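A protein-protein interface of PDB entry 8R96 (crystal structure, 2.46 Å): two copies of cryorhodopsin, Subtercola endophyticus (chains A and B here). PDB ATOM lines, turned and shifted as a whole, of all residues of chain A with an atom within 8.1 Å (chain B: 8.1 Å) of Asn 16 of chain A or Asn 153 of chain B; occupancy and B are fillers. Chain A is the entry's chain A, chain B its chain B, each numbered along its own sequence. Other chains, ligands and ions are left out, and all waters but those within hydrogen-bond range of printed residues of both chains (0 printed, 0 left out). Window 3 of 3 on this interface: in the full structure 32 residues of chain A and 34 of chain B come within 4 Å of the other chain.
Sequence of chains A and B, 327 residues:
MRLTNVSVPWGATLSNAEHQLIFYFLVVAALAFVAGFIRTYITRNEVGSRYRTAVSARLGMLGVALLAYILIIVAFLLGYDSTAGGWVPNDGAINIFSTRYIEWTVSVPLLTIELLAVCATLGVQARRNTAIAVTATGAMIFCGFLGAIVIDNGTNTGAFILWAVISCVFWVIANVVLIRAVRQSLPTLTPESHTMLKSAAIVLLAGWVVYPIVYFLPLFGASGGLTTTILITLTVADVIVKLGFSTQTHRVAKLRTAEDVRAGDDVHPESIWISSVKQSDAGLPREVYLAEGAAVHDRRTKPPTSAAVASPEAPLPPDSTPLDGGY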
ATOM      1  N   THR A  13      29.561   3.783 -11.012  1.00  0.00           N
ATOM      2  CA  THR A  13      28.201   4.209 -10.592  1.00  0.00           C
ATOM      3  C   THR A  13      27.186   3.164 -11.072  1.00  0.00           C
ATOM      4  O   THR A  13      27.362   2.641 -12.189  1.00  0.00           O
ATOM      5  CB  THR A  13      27.881   5.610 -11.126  1.00  0.00           C
ATOM      6  OG1 THR A  13      28.772   6.523 -10.486  1.00  0.00           O
ATOM      7  CG2 THR A  13      26.451   6.036 -10.877  1.00  0.00           C
ATOM      8  N   LEU A  14      26.168   2.873 -10.256  1.00  0.00           N
ATOM      9  CA  LEU A  14      25.125   1.853 -10.546  1.00  0.00           C
ATOM     10  C   LEU A  14      23.803   2.547 -10.889  1.00  0.00           C
ATOM     11  O   LEU A  14      23.472   3.550 -10.226  1.00  0.00           O
ATOM     12  CB  LEU A  14      24.945   0.951  -9.322  1.00  0.00           C
ATOM     13  CG  LEU A  14      26.196   0.218  -8.844  1.00  0.00           C
ATOM     14  CD1 LEU A  14      25.929  -0.492  -7.527  1.00  0.00           C
ATOM     15  CD2 LEU A  14      26.683  -0.767  -9.893  1.00  0.00           C
ATOM     16  N   SER A  15      23.078   2.018 -11.879  1.00  0.00           N
ATOM     17  CA  SER A  15      21.666   2.379 -12.172  1.00  0.00           C
ATOM     18  C   SER A  15      20.786   1.876 -11.022  1.00  0.00           C
ATOM     19  O   SER A  15      21.303   1.120 -10.174  1.00  0.00           O
ATOM     20  CB  SER A  15      21.217   1.815 -13.495  1.00  0.00           C
ATOM     21  OG  SER A  15      21.111   0.399 -13.433  1.00  0.00           O
ATOM     22  N   ASN A  16      19.514   2.282 -10.992  1.00  0.00           N
ATOM     23  CA  ASN A  16      18.526   1.811  -9.985  1.00  0.00           C
ATOM     24  C   ASN A  16      18.289   0.312 -10.194  1.00  0.00           C
ATOM     25  O   ASN A  16      18.285  -0.432  -9.190  1.00  0.00           O
ATOM     26  CB  ASN A  16      17.220   2.601 -10.055  1.00  0.00           C
ATOM     27  CG  ASN A  16      17.359   4.002  -9.504  1.00  0.00           C
ATOM     28  OD1 ASN A  16      18.444   4.409  -9.092  1.00  0.00           O
ATOM     29  ND2 ASN A  16      16.267   4.746  -9.490  1.00  0.00           N
ATOM     30  N   ALA A  17      18.104  -0.103 -11.451  1.00  0.00           N
ATOM     31  CA  ALA A  17      17.901  -1.512 -11.861  1.00  0.00           C
ATOM     32  C   ALA A  17      19.016  -2.378 -11.265  1.00  0.00           C
ATOM     33  O   ALA A  17      18.700  -3.424 -10.658  1.00  0.00           O
ATOM     34  CB  ALA A  17      17.872  -1.609 -13.366  1.00  0.00           C
ATOM     35  N   GLU A  18      20.270  -1.947 -11.430  1.00  0.00           N
ATOM     36  CA  GLU A  18      21.479  -2.670 -10.955  1.00  0.00           C
ATOM     37  C   GLU A  18      21.462  -2.730  -9.423  1.00  0.00           C
ATOM     38  O   GLU A  18      21.576  -3.844  -8.873  1.00  0.00           O
ATOM     39  CB  GLU A  18      22.740  -1.985 -11.490  1.00  0.00           C
ATOM     40  CG  GLU A  18      22.941  -2.177 -12.984  1.00  0.00           C
ATOM     41  CD  GLU A  18      23.948  -1.240 -13.628  1.00  0.00           C
ATOM     42  OE1 GLU A  18      24.541  -1.631 -14.653  1.00  0.00           O
ATOM     43  OE2 GLU A  18      24.133  -0.120 -13.114  1.00  0.00           O
ATOM     44  N   HIS A  19      21.315  -1.576  -8.765  1.00  0.00           N
ATOM     45  CA  HIS A  19      21.299  -1.434  -7.283  1.00  0.00           C
ATOM     46  C   HIS A  19      20.220  -2.345  -6.684  1.00  0.00           C
ATOM     47  O   HIS A  19      20.457  -2.905  -5.596  1.00  0.00           O
ATOM     48  CB  HIS A  19      21.093   0.036  -6.895  1.00  0.00           C
ATOM     49  CG  HIS A  19      21.292   0.309  -5.442  1.00  0.00           C
ATOM     50  ND1 HIS A  19      20.243   0.324  -4.542  1.00  0.00           N
ATOM     51  CD2 HIS A  19      22.407   0.581  -4.731  1.00  0.00           C
ATOM     52  CE1 HIS A  19      20.705   0.595  -3.337  1.00  0.00           C
ATOM     53  NE2 HIS A  19      22.031   0.756  -3.427  1.00  0.00           N
ATOM     54  N   GLN A  20      19.083  -2.482  -7.374  1.00  0.00           N
ATOM     55  CA  GLN A  20      17.920  -3.294  -6.926  1.00  0.00           C
ATOM     56  C   GLN A  20      18.262  -4.782  -7.075  1.00  0.00           C
ATOM     57  O   GLN A  20      17.934  -5.562  -6.158  1.00  0.00           O
ATOM     58  CB  GLN A  20      16.673  -2.925  -7.734  1.00  0.00           C
ATOM     59  CG  GLN A  20      15.365  -3.157  -6.988  1.00  0.00           C
ATOM     60  CD  GLN A  20      15.020  -2.021  -6.055  1.00  0.00           C
ATOM     61  OE1 GLN A  20      15.590  -0.935  -6.126  1.00  0.00           O
ATOM     62  NE2 GLN A  20      14.067  -2.263  -5.170  1.00  0.00           N
ATOM     63  N   LEU A  21      18.901  -5.151  -8.189  1.00  0.00           N
ATOM     64  CA  LEU A  21      19.292  -6.548  -8.519  1.00  0.00           C
ATOM     65  C   LEU A  21      20.309  -7.056  -7.491  1.00  0.00           C
ATOM     66  O   LEU A  21      20.117  -8.171  -6.974  1.00  0.00           O
ATOM     67  CB  LEU A  21      19.889  -6.585  -9.928  1.00  0.00           C
ATOM     68  CG  LEU A  21      18.884  -6.717 -11.069  1.00  0.00           C
ATOM     69  CD1 LEU A  21      19.592  -6.687 -12.414  1.00  0.00           C
ATOM     70  CD2 LEU A  21      18.062  -7.989 -10.923  1.00  0.00           C
ATOM     71  N   ILE A  22      21.356  -6.272  -7.230  1.00  0.00           N
ATOM     72  CA  ILE A  22      22.462  -6.635  -6.295  1.00  0.00           C
ATOM     73  C   ILE A  22      21.854  -6.944  -4.922  1.00  0.00           C
ATOM     74  O   ILE A  22      22.088  -8.058  -4.411  1.00  0.00           O
ATOM     75  CB  ILE A  22      23.521  -5.517  -6.224  1.00  0.00           C
ATOM     76  CG1 ILE A  22      24.201  -5.297  -7.578  1.00  0.00           C
ATOM     77  CG2 ILE A  22      24.536  -5.808  -5.129  1.00  0.00           C
ATOM     78  CD1 ILE A  22      24.963  -3.997  -7.680  1.00  0.00           C
ATOM     79  N   PHE A  23      21.092  -5.999  -4.362  1.00  0.00           N
ATOM     80  CA  PHE A  23      20.424  -6.125  -3.040  1.00  0.00           C
ATOM     81  C   PHE A  23      19.593  -7.415  -3.004  1.00  0.00           C
ATOM     82  O   PHE A  23      19.734  -8.197  -2.045  1.00  0.00           O
ATOM     83  CB  PHE A  23      19.546  -4.904  -2.756  1.00  0.00           C
ATOM     84  CG  PHE A  23      18.899  -4.907  -1.393  1.00  0.00           C
ATOM     85  CD1 PHE A  23      17.541  -5.141  -1.251  1.00  0.00           C
ATOM     86  CD2 PHE A  23      19.650  -4.681  -0.251  1.00  0.00           C
ATOM     87  CE1 PHE A  23      16.948  -5.136   0.002  1.00  0.00           C
ATOM     88  CE2 PHE A  23      19.056  -4.680   1.002  1.00  0.00           C
ATOM     89  CZ  PHE A  23      17.706  -4.908   1.126  1.00  0.00           C
ATOM     90  N   PHE A  76      26.959  -2.664   1.524  1.00  0.00           N
ATOM     91  CA  PHE A  76      26.260  -2.287   0.269  1.00  0.00           C
ATOM     92  C   PHE A  76      25.365  -1.072   0.532  1.00  0.00           C
ATOM     93  O   PHE A  76      25.394  -0.120  -0.276  1.00  0.00           O
ATOM     94  CB  PHE A  76      25.445  -3.463  -0.275  1.00  0.00           C
ATOM     95  CG  PHE A  76      24.589  -3.125  -1.470  1.00  0.00           C
ATOM     96  CD1 PHE A  76      23.228  -2.898  -1.327  1.00  0.00           C
ATOM     97  CD2 PHE A  76      25.145  -3.018  -2.734  1.00  0.00           C
ATOM     98  CE1 PHE A  76      22.441  -2.582  -2.424  1.00  0.00           C
ATOM     99  CE2 PHE A  76      24.358  -2.697  -3.829  1.00  0.00           C
ATOM    100  CZ  PHE A  76      23.008  -2.480  -3.674  1.00  0.00           C
ATOM    101  N   ASP A  81      25.455   6.214  -2.525  1.00  0.00           N
ATOM    102  CA  ASP A  81      24.515   7.334  -2.255  1.00  0.00           C
ATOM    103  C   ASP A  81      23.692   7.588  -3.520  1.00  0.00           C
ATOM    104  O   ASP A  81      24.293   7.668  -4.610  1.00  0.00           O
ATOM    105  CB  ASP A  81      25.260   8.594  -1.807  1.00  0.00           C
ATOM    106  CG  ASP A  81      26.402   8.312  -0.847  1.00  0.00           C
ATOM    107  OD1 ASP A  81      27.479   7.902  -1.324  1.00  0.00           O
ATOM    108  OD2 ASP A  81      26.198   8.488   0.371  1.00  0.00           O
ATOM    109  N   SER A  82      22.367   7.691  -3.379  1.00  0.00           N
ATOM    110  CA  SER A  82      21.420   7.931  -4.498  1.00  0.00           C
ATOM    111  C   SER A  82      21.546   9.383  -4.967  1.00  0.00           C
ATOM    112  O   SER A  82      21.563  10.286  -4.110  1.00  0.00           O
ATOM    113  CB  SER A  82      20.009   7.602  -4.104  1.00  0.00           C
ATOM    114  OG  SER A  82      19.166   7.567  -5.246  1.00  0.00           O
ATOM    115  N   THR A  83      21.640   9.585  -6.284  1.00  0.00           N
ATOM    116  CA  THR A  83      21.790  10.908  -6.945  1.00  0.00           C
ATOM    117  C   THR A  83      20.889  10.943  -8.184  1.00  0.00           C
ATOM    118  O   THR A  83      20.147   9.964  -8.400  1.00  0.00           O
ATOM    119  CB  THR A  83      23.255  11.174  -7.313  1.00  0.00           C
ATOM    120  OG1 THR A  83      23.635  10.244  -8.329  1.00  0.00           O
ATOM    121  CG2 THR A  83      24.197  11.046  -6.136  1.00  0.00           C
ATOM    122  N   ALA A  84      20.958  12.026  -8.962  1.00  0.00           N
ATOM    123  CA  ALA A  84      20.249  12.188 -10.253  1.00  0.00           C
ATOM    124  C   ALA A  84      20.833  11.204 -11.274  1.00  0.00           C
ATOM    125  O   ALA A  84      20.134  10.885 -12.255  1.00  0.00           O
ATOM    126  CB  ALA A  84      20.366  13.614 -10.731  1.00  0.00           C
ATOM    127  N   GLY A  85      22.064  10.740 -11.033  1.00  0.00           N
ATOM    128  CA  GLY A  85      22.840   9.907 -11.973  1.00  0.00           C
ATOM    129  C   GLY A  85      22.808   8.434 -11.602  1.00  0.00           C
ATOM    130  O   GLY A  85      23.525   7.650 -12.257  1.00  0.00           O
ATOM    131  N   GLY A  86      22.012   8.069 -10.591  1.00  0.00           N
ATOM    132  CA  GLY A  86      21.841   6.676 -10.127  1.00  0.00           C
ATOM    133  C   GLY A  86      22.314   6.494  -8.695  1.00  0.00           C
ATOM    134  O   GLY A  86      21.794   7.201  -7.814  1.00  0.00           O
ATOM    135  N   TRP A  87      23.257   5.571  -8.471  1.00  0.00           N
ATOM    136  CA  TRP A  87      23.876   5.283  -7.148  1.00  0.00           C
ATOM    137  C   TRP A  87      25.393   5.470  -7.247  1.00  0.00           C
ATOM    138  O   TRP A  87      26.056   4.636  -7.895  1.00  0.00           O
ATOM    139  CB  TRP A  87      23.503   3.872  -6.670  1.00  0.00           C
ATOM    140  CG  TRP A  87      22.065   3.732  -6.280  1.00  0.00           C
ATOM    141  CD1 TRP A  87      21.017   3.416  -7.095  1.00  0.00           C
ATOM    142  CD2 TRP A  87      21.504   3.923  -4.968  1.00  0.00           C
ATOM    143  NE1 TRP A  87      19.848   3.390  -6.382  1.00  0.00           N
ATOM    144  CE2 TRP A  87      20.116   3.695  -5.074  1.00  0.00           C
ATOM    145  CE3 TRP A  87      22.039   4.253  -3.717  1.00  0.00           C
ATOM    146  CZ2 TRP A  87      19.260   3.791  -3.979  1.00  0.00           C
ATOM    147  CZ3 TRP A  87      21.192   4.348  -2.634  1.00  0.00           C
ATOM    148  CH2 TRP A  87      19.823   4.121  -2.767  1.00  0.00           C
ATOM    149  N   VAL B   6       2.183   2.391 -16.195  1.00  0.00           N
ATOM    150  CA  VAL B   6       1.700   1.580 -15.035  1.00  0.00           C
ATOM    151  C   VAL B   6       1.727   2.455 -13.776  1.00  0.00           C
ATOM    152  O   VAL B   6       2.795   3.033 -13.491  1.00  0.00           O
ATOM    153  CB  VAL B   6       2.557   0.312 -14.850  1.00  0.00           C
ATOM    154  CG1 VAL B   6       2.208  -0.436 -13.572  1.00  0.00           C
ATOM    155  CG2 VAL B   6       2.460  -0.620 -16.048  1.00  0.00           C
ATOM    156  N   VAL B   8       2.416   2.720 -10.414  1.00  0.00           N
ATOM    157  CA  VAL B   8       3.205   2.066  -9.327  1.00  0.00           C
ATOM    158  C   VAL B   8       2.521   2.349  -7.992  1.00  0.00           C
ATOM    159  O   VAL B   8       2.150   3.484  -7.701  1.00  0.00           O
ATOM    160  CB  VAL B   8       4.671   2.541  -9.327  1.00  0.00           C
ATOM    161  CG1 VAL B   8       5.405   2.094 -10.582  1.00  0.00           C
ATOM    162  CG2 VAL B   8       4.776   4.047  -9.143  1.00  0.00           C
ATOM    163  N   PRO B   9       2.335   1.313  -7.143  1.00  0.00           N
ATOM    164  CA  PRO B   9       1.596   1.452  -5.888  1.00  0.00           C
ATOM    165  C   PRO B   9       2.349   2.261  -4.820  1.00  0.00           C
ATOM    166  O   PRO B   9       1.715   2.712  -3.884  1.00  0.00           O
ATOM    167  CB  PRO B   9       1.409   0.006  -5.395  1.00  0.00           C
ATOM    168  CG  PRO B   9       1.825  -0.878  -6.563  1.00  0.00           C
ATOM    169  CD  PRO B   9       2.817  -0.058  -7.356  1.00  0.00           C
ATOM    170  N   TRP B  10       3.666   2.415  -4.979  1.00  0.00           N
ATOM    171  CA  TRP B  10       4.546   3.161  -4.039  1.00  0.00           C
ATOM    172  C   TRP B  10       4.573   4.649  -4.412  1.00  0.00           C
ATOM    173  O   TRP B  10       5.453   5.372  -3.903  1.00  0.00           O
ATOM    174  CB  TRP B  10       5.954   2.554  -4.013  1.00  0.00           C
ATOM    175  CG  TRP B  10       6.593   2.409  -5.359  1.00  0.00           C
ATOM    176  CD1 TRP B  10       7.292   3.359  -6.043  1.00  0.00           C
ATOM    177  CD2 TRP B  10       6.611   1.227  -6.181  1.00  0.00           C
ATOM    178  NE1 TRP B  10       7.743   2.853  -7.233  1.00  0.00           N
ATOM    179  CE2 TRP B  10       7.339   1.547  -7.346  1.00  0.00           C
ATOM    180  CE3 TRP B  10       6.088  -0.065  -6.048  1.00  0.00           C
ATOM    181  CZ2 TRP B  10       7.549   0.623  -8.369  1.00  0.00           C
ATOM    182  CZ3 TRP B  10       6.301  -0.977  -7.059  1.00  0.00           C
ATOM    183  CH2 TRP B  10       7.020  -0.635  -8.204  1.00  0.00           C
ATOM    184  N   ASP B  91      11.564   7.758  -1.714  1.00  0.00           N
ATOM    185  CA  ASP B  91      12.272   6.932  -2.727  1.00  0.00           C
ATOM    186  C   ASP B  91      12.282   5.466  -2.286  1.00  0.00           C
ATOM    187  O   ASP B  91      12.279   4.594  -3.171  1.00  0.00           O
ATOM    188  CB  ASP B  91      13.694   7.446  -2.967  1.00  0.00           C
ATOM    189  CG  ASP B  91      13.733   8.792  -3.669  1.00  0.00           C
ATOM    190  OD1 ASP B  91      12.653   9.392  -3.845  1.00  0.00           O
ATOM    191  OD2 ASP B  91      14.842   9.226  -4.038  1.00  0.00           O
ATOM    192  N   ILE B  94       9.273   1.912  -2.642  1.00  0.00           N
ATOM    193  CA  ILE B  94       9.301   0.777  -3.612  1.00  0.00           C
ATOM    194  C   ILE B  94       9.857  -0.462  -2.899  1.00  0.00           C
ATOM    195  O   ILE B  94       9.432  -1.579  -3.247  1.00  0.00           O
ATOM    196  CB  ILE B  94      10.126   1.126  -4.868  1.00  0.00           C
ATOM    197  CG1 ILE B  94      10.130  -0.024  -5.878  1.00  0.00           C
ATOM    198  CG2 ILE B  94      11.535   1.547  -4.489  1.00  0.00           C
ATOM    199  CD1 ILE B  94      10.911   0.257  -7.139  1.00  0.00           C
ATOM    200  N   PHE B 145       9.474 -10.023 -10.461  1.00  0.00           N
ATOM    201  CA  PHE B 145      10.385  -9.007  -9.871  1.00  0.00           C
ATOM    202  C   PHE B 145      10.895  -8.075 -10.974  1.00  0.00           C
ATOM    203  O   PHE B 145      10.834  -6.841 -10.795  1.00  0.00           O
ATOM    204  CB  PHE B 145      11.544  -9.683  -9.132  1.00  0.00           C
ATOM    205  CG  PHE B 145      12.514  -8.730  -8.476  1.00  0.00           C
ATOM    206  CD1 PHE B 145      13.857  -8.739  -8.814  1.00  0.00           C
ATOM    207  CD2 PHE B 145      12.080  -7.814  -7.530  1.00  0.00           C
ATOM    208  CE1 PHE B 145      14.747  -7.861  -8.213  1.00  0.00           C
ATOM    209  CE2 PHE B 145      12.971  -6.938  -6.928  1.00  0.00           C
ATOM    210  CZ  PHE B 145      14.302  -6.962  -7.271  1.00  0.00           C
ATOM    211  N   LEU B 146      11.377  -8.651 -12.079  1.00  0.00           N
ATOM    212  CA  LEU B 146      11.900  -7.902 -13.254  1.00  0.00           C
ATOM    213  C   LEU B 146      10.806  -6.971 -13.793  1.00  0.00           C
ATOM    214  O   LEU B 146      11.097  -5.779 -14.020  1.00  0.00           O
ATOM    215  CB  LEU B 146      12.356  -8.897 -14.326  1.00  0.00           C
ATOM    216  CG  LEU B 146      13.651  -9.653 -14.023  1.00  0.00           C
ATOM    217  CD1 LEU B 146      14.021 -10.574 -15.173  1.00  0.00           C
ATOM    218  CD2 LEU B 146      14.794  -8.695 -13.724  1.00  0.00           C
ATOM    219  N   GLY B 147       9.593  -7.502 -13.976  1.00  0.00           N
ATOM    220  CA  GLY B 147       8.444  -6.777 -14.548  1.00  0.00           C
ATOM    221  C   GLY B 147       8.009  -5.609 -13.679  1.00  0.00           C
ATOM    222  O   GLY B 147       7.929  -4.483 -14.203  1.00  0.00           O
ATOM    223  N   ALA B 148       7.748  -5.865 -12.395  1.00  0.00           N
ATOM    224  CA  ALA B 148       7.042  -4.948 -11.470  1.00  0.00           C
ATOM    225  C   ALA B 148       8.013  -3.950 -10.826  1.00  0.00           C
ATOM    226  O   ALA B 148       7.542  -2.871 -10.411  1.00  0.00           O
ATOM    227  CB  ALA B 148       6.315  -5.749 -10.418  1.00  0.00           C
ATOM    228  N   ILE B 149       9.304  -4.289 -10.738  1.00  0.00           N
ATOM    229  CA  ILE B 149      10.295  -3.540  -9.908  1.00  0.00           C
ATOM    230  C   ILE B 149      11.496  -3.108 -10.758  1.00  0.00           C
ATOM    231  O   ILE B 149      11.705  -1.889 -10.904  1.00  0.00           O
ATOM    232  CB  ILE B 149      10.744  -4.388  -8.699  1.00  0.00           C
ATOM    233  CG1 ILE B 149       9.574  -4.722  -7.771  1.00  0.00           C
ATOM    234  CG2 ILE B 149      11.873  -3.701  -7.948  1.00  0.00           C
ATOM    235  CD1 ILE B 149       9.086  -3.552  -6.943  1.00  0.00           C
ATOM    236  N   VAL B 150      12.263  -4.071 -11.275  1.00  0.00           N
ATOM    237  CA  VAL B 150      13.641  -3.858 -11.813  1.00  0.00           C
ATOM    238  C   VAL B 150      13.583  -2.994 -13.081  1.00  0.00           C
ATOM    239  O   VAL B 150      14.251  -1.939 -13.105  1.00  0.00           O
ATOM    240  CB  VAL B 150      14.347  -5.199 -12.080  1.00  0.00           C
ATOM    241  CG1 VAL B 150      15.733  -4.997 -12.672  1.00  0.00           C
ATOM    242  CG2 VAL B 150      14.418  -6.056 -10.824  1.00  0.00           C
ATOM    243  N   ILE B 151      12.824  -3.430 -14.091  1.00  0.00           N
ATOM    244  CA  ILE B 151      12.813  -2.834 -15.462  1.00  0.00           C
ATOM    245  C   ILE B 151      12.110  -1.471 -15.427  1.00  0.00           C
ATOM    246  O   ILE B 151      10.895  -1.437 -15.150  1.00  0.00           O
ATOM    247  CB  ILE B 151      12.148  -3.795 -16.466  1.00  0.00           C
ATOM    248  CG1 ILE B 151      12.957  -5.082 -16.634  1.00  0.00           C
ATOM    249  CG2 ILE B 151      11.913  -3.102 -17.800  1.00  0.00           C
ATOM    250  CD1 ILE B 151      12.288  -6.117 -17.505  1.00  0.00           C
ATOM    251  N   ASP B 152      12.856  -0.399 -15.714  1.00  0.00           N
ATOM    252  CA  ASP B 152      12.344   0.994 -15.818  1.00  0.00           C
ATOM    253  C   ASP B 152      11.498   1.315 -14.580  1.00  0.00           C
ATOM    254  O   ASP B 152      10.401   1.885 -14.742  1.00  0.00           O
ATOM    255  CB  ASP B 152      11.556   1.193 -17.117  1.00  0.00           C
ATOM    256  CG  ASP B 152      12.364   0.906 -18.374  1.00  0.00           C
ATOM    257  OD1 ASP B 152      13.562   1.254 -18.396  1.00  0.00           O
ATOM    258  OD2 ASP B 152      11.790   0.330 -19.320  1.00  0.00           O
ATOM    259  N   ASN B 153      11.997   0.948 -13.396  1.00  0.00           N
ATOM    260  CA  ASN B 153      11.378   1.249 -12.075  1.00  0.00           C
ATOM    261  C   ASN B 153       9.926   0.761 -12.053  1.00  0.00           C
ATOM    262  O   ASN B 153       9.135   1.319 -11.271  1.00  0.00           O
ATOM    263  CB  ASN B 153      11.459   2.741 -11.749  1.00  0.00           C
ATOM    264  CG  ASN B 153      12.855   3.294 -11.920  1.00  0.00           C
ATOM    265  OD1 ASN B 153      13.833   2.556 -11.827  1.00  0.00           O
ATOM    266  ND2 ASN B 153      12.956   4.586 -12.179  1.00  0.00           N
ATOM    267  N   GLY B 154       9.600  -0.238 -12.881  1.00  0.00           N
ATOM    268  CA  GLY B 154       8.284  -0.907 -12.906  1.00  0.00           C
ATOM    269  C   GLY B 154       7.185  -0.003 -13.436  1.00  0.00           C
ATOM    270  O   GLY B 154       6.024  -0.178 -13.014  1.00  0.00           O
ATOM    271  N   THR B 155       7.533   0.926 -14.331  1.00  0.00           N
ATOM    272  CA  THR B 155       6.597   1.897 -14.958  1.00  0.00           C
ATOM    273  C   THR B 155       6.255   1.432 -16.379  1.00  0.00           C
ATOM    274  O   THR B 155       5.146   1.747 -16.856  1.00  0.00           O
ATOM    275  CB  THR B 155       7.187   3.312 -14.945  1.00  0.00           C
ATOM    276  OG1 THR B 155       8.457   3.272 -15.598  1.00  0.00           O
ATOM    277  CG2 THR B 155       7.351   3.867 -13.547  1.00  0.00           C
ATOM    278  N   ASN B 156       7.176   0.702 -17.017  1.00  0.00           N
ATOM    279  CA  ASN B 156       7.037   0.170 -18.400  1.00  0.00           C
ATOM    280  C   ASN B 156       5.932  -0.895 -18.423  1.00  0.00           C
ATOM    281  O   ASN B 156       6.171  -2.005 -17.906  1.00  0.00           O
ATOM    282  CB  ASN B 156       8.371  -0.380 -18.911  1.00  0.00           C
ATOM    283  CG  ASN B 156       8.266  -1.024 -20.276  1.00  0.00           C
ATOM    284  OD1 ASN B 156       7.192  -1.465 -20.681  1.00  0.00           O
ATOM    285  ND2 ASN B 156       9.377  -1.090 -20.989  1.00  0.00           N
ATOM    286  N   PHE B 160       6.105  -5.088 -17.798  1.00  0.00           N
ATOM    287  CA  PHE B 160       5.186  -5.401 -16.673  1.00  0.00           C
ATOM    288  C   PHE B 160       4.305  -6.594 -17.056  1.00  0.00           C
ATOM    289  O   PHE B 160       4.210  -7.551 -16.263  1.00  0.00           O
ATOM    290  CB  PHE B 160       4.343  -4.174 -16.320  1.00  0.00           C
ATOM    291  CG  PHE B 160       3.502  -4.321 -15.078  1.00  0.00           C
ATOM    292  CD1 PHE B 160       2.170  -4.694 -15.161  1.00  0.00           C
ATOM    293  CD2 PHE B 160       4.040  -4.075 -13.824  1.00  0.00           C
ATOM    294  CE1 PHE B 160       1.397  -4.822 -14.018  1.00  0.00           C
ATOM    295  CE2 PHE B 160       3.266  -4.206 -12.681  1.00  0.00           C
ATOM    296  CZ  PHE B 160       1.946  -4.580 -12.781  1.00  0.00           C
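The side-chain amide oxygen (OD1) of Asn 16 of chain A lies within hydrogen-bond range of the indole nitrogen (NE1) of Trp 87 of chain A, 3.2 Å away.
The backbone carbonyl oxygen (O) of Phe 145 of chain B is in hydrogen-bond range of the backbone NH (N) of Val 150 of chain B, 3.2 Å away.
O of Ile 149 of chain B lies within hydrogen-bond range of N of Gly 154 of chain B (3.3 Å).
Among the printed residues, merely in contact across the chains: Ala 17 of chain A with Val 150 of chain B (3.6 Å), Gln 20 of chain A with Ile 149 of chain B (3.7 Å), Asn 16 of chain A with Asn 153 of chain B (3.8 Å), Leu 21 of chain A with Val 150 of chain B (3.9 Å) and Gln 20 of chain A with Phe 145 of chain B (3.96 Å).
Of chain B, only Asn 153 (3.8 Å) comes within 4 Å of Asn 16 of chain A.
Asn 153 of chain B touches just one residue of chain A: Asn 16.
No residue of chain A comes within 4 Å of Gly 154 of chain B.
Printed residues of chain B within 4 Å of Leu 21 of chain A: Val 150 (3.9 Å).
Printed residues of chain B within 4 Å of Gln 20 of chain A: Phe 145 (3.96 Å) and Ile 149 (3.7 Å).
Printed residues of chain A within 4 Å of Val 150 of chain B: Ala 17 (3.6 Å) and Leu 21 (3.9 Å).
Of the printed residues of chain A, Phe 145 of chain B touches Gln 20 (3.96 Å).
His 19 of chain A touches none of the printed residues of chain B.
Along chain A the printed residues that touch a printed residue of chain B span positions 16 to 21.
Among the printed residues, 5 pairs touch across the chains.
Among the printed residues, no Asp or Glu carboxylate lies within 4 Å of a Lys or Arg side-chain nitrogen of the other chain.
No position is printed for both chains.
Of the 5 pairs that touch across the chains among the printed residues, none has its exchanged pair printed and touching as well.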
